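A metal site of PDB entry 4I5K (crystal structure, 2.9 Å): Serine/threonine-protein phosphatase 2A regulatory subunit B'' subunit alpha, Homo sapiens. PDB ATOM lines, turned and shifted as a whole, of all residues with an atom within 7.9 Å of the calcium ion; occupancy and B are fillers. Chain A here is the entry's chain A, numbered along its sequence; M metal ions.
OD1 of Asp 137 is in salt-bridge range of NH2 of Arg 140, at 2.9 Å.
O of Asp 126 is in hydrogen-bond range of ND1 of His 129 (3.0 Å).
The side-chain carboxylate of Asp 137 lies within hydrogen-bond range of the side-chain hydroxyl of Thr 127, 2.5 Å away.
OD2 of Asp 126 lies within hydrogen-bond range of N of Leu 131 (2.7 Å).
The guanidinium group (NH2) of Arg 140 sits close to the side-chain carboxylate (OD2) of Asp 128.
OG of Ser 134 lies within hydrogen-bond range of N of Asp 137, 3.1 Å away.
NH2 of Arg 170 is in salt-bridge range of OD2 of Asp 130, at 2.4 Å.
Of the 18 residues printed, 5 come within 4 Å of the calcium ion.
Along chain A the residues within 4 Å of the calcium ion span positions 126 to 137.
The nearest printed residue that does not touch the calcium ion is His 129 (4.4 Å).
The calcium ion is bound by the side-chain carboxylate (OD1) of Asp 130 (2.1 Å), the side-chain carboxylate (OD1) of Asp 126 (2.2 Å), the backbone carbonyl oxygen (O) of Tyr 132 (2.3 Å), the side-chain carboxylate (OD2) of Asp 128 (2.3 Å) and the side-chain carboxylate (OD2) of Asp 137 (2.3 Å).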
ATOM      1  N   PHE A 122       7.791  19.336  13.260  1.00  0.00           N
ATOM      2  CA  PHE A 122       8.098  19.729  11.893  1.00  0.00           C
ATOM      3  C   PHE A 122       8.189  18.479  11.030  1.00  0.00           C
ATOM      4  O   PHE A 122       7.678  18.434   9.916  1.00  0.00           O
ATOM      5  CB  PHE A 122       9.426  20.489  11.847  1.00  0.00           C
ATOM      6  CG  PHE A 122       9.922  20.768  10.460  1.00  0.00           C
ATOM      7  CD1 PHE A 122       9.373  21.804   9.709  1.00  0.00           C
ATOM      8  CD2 PHE A 122      10.930  19.998   9.899  1.00  0.00           C
ATOM      9  CE1 PHE A 122       9.829  22.077   8.433  1.00  0.00           C
ATOM     10  CE2 PHE A 122      11.381  20.258   8.622  1.00  0.00           C
ATOM     11  CZ  PHE A 122      10.833  21.301   7.883  1.00  0.00           C
ATOM     12  N   LEU A 125       4.761  16.787  10.351  1.00  0.00           N
ATOM     13  CA  LEU A 125       3.909  17.492   9.389  1.00  0.00           C
ATOM     14  C   LEU A 125       4.381  17.383   7.936  1.00  0.00           C
ATOM     15  O   LEU A 125       3.556  17.390   7.027  1.00  0.00           O
ATOM     16  CB  LEU A 125       3.778  18.976   9.755  1.00  0.00           C
ATOM     17  CG  LEU A 125       3.240  19.368  11.136  1.00  0.00           C
ATOM     18  CD1 LEU A 125       2.920  20.839  11.171  1.00  0.00           C
ATOM     19  CD2 LEU A 125       2.036  18.561  11.509  1.00  0.00           C
ATOM     20  N   ASP A 126       5.690  17.307   7.739  1.00  0.00           N
ATOM     21  CA  ASP A 126       6.257  17.272   6.392  1.00  0.00           C
ATOM     22  C   ASP A 126       5.895  15.960   5.709  1.00  0.00           C
ATOM     23  O   ASP A 126       6.750  15.102   5.478  1.00  0.00           O
ATOM     24  CB  ASP A 126       7.779  17.413   6.481  1.00  0.00           C
ATOM     25  CG  ASP A 126       8.431  17.655   5.134  1.00  0.00           C
ATOM     26  OD1 ASP A 126       7.771  18.218   4.247  1.00  0.00           O
ATOM     27  OD2 ASP A 126       9.615  17.291   4.978  1.00  0.00           O
ATOM     28  N   THR A 127       4.614  15.819   5.361  1.00  0.00           N
ATOM     29  CA  THR A 127       4.062  14.578   4.824  1.00  0.00           C
ATOM     30  C   THR A 127       4.627  14.228   3.450  1.00  0.00           C
ATOM     31  O   THR A 127       4.740  13.042   3.129  1.00  0.00           O
ATOM     32  CB  THR A 127       2.522  14.591   4.791  1.00  0.00           C
ATOM     33  OG1 THR A 127       2.041  15.898   4.469  1.00  0.00           O
ATOM     34  CG2 THR A 127       1.956  14.181   6.148  1.00  0.00           C
ATOM     35  N   ASP A 128       4.957  15.225   2.636  1.00  0.00           N
ATOM     36  CA  ASP A 128       5.579  14.956   1.344  1.00  0.00           C
ATOM     37  C   ASP A 128       7.129  14.862   1.410  1.00  0.00           C
ATOM     38  O   ASP A 128       7.789  14.663   0.390  1.00  0.00           O
ATOM     39  CB  ASP A 128       5.099  15.916   0.243  1.00  0.00           C
ATOM     40  CG  ASP A 128       5.356  17.375   0.544  1.00  0.00           C
ATOM     41  OD1 ASP A 128       5.989  18.044  -0.305  1.00  0.00           O
ATOM     42  OD2 ASP A 128       4.944  17.872   1.612  1.00  0.00           O
ATOM     43  N   HIS A 129       7.680  14.963   2.620  1.00  0.00           N
ATOM     44  CA  HIS A 129       9.112  14.782   2.885  1.00  0.00           C
ATOM     45  C   HIS A 129      10.091  15.697   2.136  1.00  0.00           C
ATOM     46  O   HIS A 129      11.264  15.343   1.999  1.00  0.00           O
ATOM     47  CB  HIS A 129       9.509  13.318   2.584  1.00  0.00           C
ATOM     48  CG  HIS A 129       8.700  12.295   3.337  1.00  0.00           C
ATOM     49  ND1 HIS A 129       7.596  12.616   4.094  1.00  0.00           N
ATOM     50  CD2 HIS A 129       8.792  10.942   3.353  1.00  0.00           C
ATOM     51  CE1 HIS A 129       7.073  11.501   4.601  1.00  0.00           C
ATOM     52  NE2 HIS A 129       7.774  10.475   4.158  1.00  0.00           N
ATOM     53  N   ASP A 130       9.654  16.872   1.703  1.00  0.00           N
ATOM     54  CA  ASP A 130      10.526  17.781   0.949  1.00  0.00           C
ATOM     55  C   ASP A 130      11.254  18.776   1.843  1.00  0.00           C
ATOM     56  O   ASP A 130      11.941  19.665   1.338  1.00  0.00           O
ATOM     57  CB  ASP A 130       9.748  18.554  -0.103  1.00  0.00           C
ATOM     58  CG  ASP A 130       8.633  19.361   0.487  1.00  0.00           C
ATOM     59  OD1 ASP A 130       8.203  19.026   1.610  1.00  0.00           O
ATOM     60  OD2 ASP A 130       8.183  20.333  -0.158  1.00  0.00           O
ATOM     61  N   LEU A 131      11.069  18.643   3.153  1.00  0.00           N
ATOM     62  CA  LEU A 131      11.694  19.527   4.153  1.00  0.00           C
ATOM     63  C   LEU A 131      11.137  20.957   4.172  1.00  0.00           C
ATOM     64  O   LEU A 131      11.769  21.876   4.697  1.00  0.00           O
ATOM     65  CB  LEU A 131      13.214  19.493   3.974  1.00  0.00           C
ATOM     66  CG  LEU A 131      13.730  18.061   4.135  1.00  0.00           C
ATOM     67  CD1 LEU A 131      15.172  17.940   3.711  1.00  0.00           C
ATOM     68  CD2 LEU A 131      13.551  17.619   5.575  1.00  0.00           C
ATOM     69  N   TYR A 132       9.956  21.130   3.595  1.00  0.00           N
ATOM     70  CA  TYR A 132       9.222  22.388   3.687  1.00  0.00           C
ATOM     71  C   TYR A 132       7.791  22.086   4.052  1.00  0.00           C
ATOM     72  O   TYR A 132       7.246  21.045   3.673  1.00  0.00           O
ATOM     73  CB  TYR A 132       9.252  23.150   2.362  1.00  0.00           C
ATOM     74  CG  TYR A 132      10.551  23.864   2.102  1.00  0.00           C
ATOM     75  CD1 TYR A 132      11.672  23.175   1.674  1.00  0.00           C
ATOM     76  CD2 TYR A 132      10.649  25.245   2.249  1.00  0.00           C
ATOM     77  CE1 TYR A 132      12.858  23.839   1.425  1.00  0.00           C
ATOM     78  CE2 TYR A 132      11.836  25.910   2.000  1.00  0.00           C
ATOM     79  CZ  TYR A 132      12.923  25.202   1.584  1.00  0.00           C
ATOM     80  OH  TYR A 132      14.105  25.853   1.334  1.00  0.00           O
ATOM     81  N   ILE A 133       7.143  23.019   4.756  1.00  0.00           N
ATOM     82  CA  ILE A 133       5.742  22.842   5.101  1.00  0.00           C
ATOM     83  C   ILE A 133       4.900  23.613   4.104  1.00  0.00           C
ATOM     84  O   ILE A 133       5.021  24.834   3.973  1.00  0.00           O
ATOM     85  CB  ILE A 133       5.447  23.370   6.528  1.00  0.00           C
ATOM     86  CG1 ILE A 133       6.367  22.720   7.560  1.00  0.00           C
ATOM     87  CG2 ILE A 133       3.979  23.150   6.886  1.00  0.00           C
ATOM     88  CD1 ILE A 133       6.227  21.208   7.622  1.00  0.00           C
ATOM     89  N   SER A 134       4.065  22.883   3.383  1.00  0.00           N
ATOM     90  CA  SER A 134       3.135  23.487   2.448  1.00  0.00           C
ATOM     91  C   SER A 134       1.771  23.643   3.103  1.00  0.00           C
ATOM     92  O   SER A 134       1.553  23.215   4.235  1.00  0.00           O
ATOM     93  CB  SER A 134       3.007  22.639   1.182  1.00  0.00           C
ATOM     94  OG  SER A 134       2.429  21.373   1.476  1.00  0.00           O
ATOM     95  N   GLN A 135       0.852  24.256   2.371  1.00  0.00           N
ATOM     96  CA  GLN A 135      -0.521  24.410   2.837  1.00  0.00           C
ATOM     97  C   GLN A 135      -1.203  23.037   2.883  1.00  0.00           C
ATOM     98  O   GLN A 135      -2.031  22.768   3.753  1.00  0.00           O
ATOM     99  CB  GLN A 135      -1.260  25.365   1.910  1.00  0.00           C
ATOM    100  CG  GLN A 135      -2.436  26.066   2.529  1.00  0.00           C
ATOM    101  CD  GLN A 135      -2.555  27.490   2.029  1.00  0.00           C
ATOM    102  OE1 GLN A 135      -1.739  27.948   1.220  1.00  0.00           O
ATOM    103  NE2 GLN A 135      -3.584  28.189   2.493  1.00  0.00           N
ATOM    104  N   ALA A 136      -0.795  22.172   1.961  1.00  0.00           N
ATOM    105  CA  ALA A 136      -1.349  20.821   1.834  1.00  0.00           C
ATOM    106  C   ALA A 136      -0.900  19.922   2.977  1.00  0.00           C
ATOM    107  O   ALA A 136      -1.642  19.049   3.422  1.00  0.00           O
ATOM    108  CB  ALA A 136      -0.949  20.205   0.494  1.00  0.00           C
ATOM    109  N   ASP A 137       0.336  20.127   3.431  1.00  0.00           N
ATOM    110  CA  ASP A 137       0.889  19.366   4.542  1.00  0.00           C
ATOM    111  C   ASP A 137       0.054  19.503   5.808  1.00  0.00           C
ATOM    112  O   ASP A 137      -0.088  18.546   6.571  1.00  0.00           O
ATOM    113  CB  ASP A 137       2.316  19.833   4.835  1.00  0.00           C
ATOM    114  CG  ASP A 137       3.338  19.141   3.975  1.00  0.00           C
ATOM    115  OD1 ASP A 137       3.093  17.975   3.598  1.00  0.00           O
ATOM    116  OD2 ASP A 137       4.363  19.762   3.649  1.00  0.00           O
ATOM    117  N   LEU A 138      -0.477  20.696   6.021  1.00  0.00           N
ATOM    118  CA  LEU A 138      -1.273  20.966   7.206  1.00  0.00           C
ATOM    119  C   LEU A 138      -2.648  20.298   7.103  1.00  0.00           C
ATOM    120  O   LEU A 138      -3.184  19.804   8.093  1.00  0.00           O
ATOM    121  CB  LEU A 138      -1.428  22.467   7.405  1.00  0.00           C
ATOM    122  CG  LEU A 138      -0.077  23.161   7.641  1.00  0.00           C
ATOM    123  CD1 LEU A 138      -0.252  24.633   7.969  1.00  0.00           C
ATOM    124  CD2 LEU A 138       0.754  22.445   8.691  1.00  0.00           C
ATOM    125  N   ARG A 140      -3.226  17.550   5.359  1.00  0.00           N
ATOM    126  CA  ARG A 140      -3.053  16.099   5.380  1.00  0.00           C
ATOM    127  C   ARG A 140      -2.692  15.561   6.765  1.00  0.00           C
ATOM    128  O   ARG A 140      -2.825  14.368   7.035  1.00  0.00           O
ATOM    129  CB  ARG A 140      -2.014  15.665   4.343  1.00  0.00           C
ATOM    130  CG  ARG A 140      -2.541  15.762   2.915  1.00  0.00           C
ATOM    131  CD  ARG A 140      -1.497  15.418   1.862  1.00  0.00           C
ATOM    132  NE  ARG A 140      -0.280  16.225   2.009  1.00  0.00           N
ATOM    133  CZ  ARG A 140       0.569  16.461   1.018  1.00  0.00           C
ATOM    134  NH1 ARG A 140       0.341  15.978  -0.192  1.00  0.00           N
ATOM    135  NH2 ARG A 140       1.659  17.198   1.235  1.00  0.00           N
ATOM    136  N   ARG A 170       5.466  27.956   0.300  1.00  0.00           N
ATOM    137  CA  ARG A 170       6.242  27.065   1.166  1.00  0.00           C
ATOM    138  C   ARG A 170       6.732  27.736   2.425  1.00  0.00           C
ATOM    139  O   ARG A 170       7.376  28.785   2.368  1.00  0.00           O
ATOM    140  CB  ARG A 170       7.448  26.504   0.416  1.00  0.00           C
ATOM    141  CG  ARG A 170       7.164  25.429  -0.607  1.00  0.00           C
ATOM    142  CD  ARG A 170       8.493  24.887  -1.129  1.00  0.00           C
ATOM    143  NE  ARG A 170       8.505  23.435  -1.279  1.00  0.00           N
ATOM    144  CZ  ARG A 170       9.534  22.751  -1.751  1.00  0.00           C
ATOM    145  NH1 ARG A 170      10.644  23.389  -2.116  1.00  0.00           N
ATOM    146  NH2 ARG A 170       9.474  21.431  -1.868  1.00  0.00           N
ATOM    147  N   MET A 171       6.468  27.121   3.570  1.00  0.00           N
ATOM    148  CA  MET A 171       6.927  27.645   4.845  1.00  0.00           C
ATOM    149  C   MET A 171       8.210  26.929   5.267  1.00  0.00           C
ATOM    150  O   MET A 171       8.235  25.714   5.440  1.00  0.00           O
ATOM    151  CB  MET A 171       5.842  27.446   5.906  1.00  0.00           C
ATOM    152  CG  MET A 171       6.306  27.712   7.324  1.00  0.00           C
ATOM    153  SD  MET A 171       5.078  27.183   8.506  1.00  0.00           S
ATOM    154  CE  MET A 171       3.800  28.413   8.294  1.00  0.00           C
HETATM  155 CA    CA M   1       6.427  19.135   2.771  1.00  0.00          CA
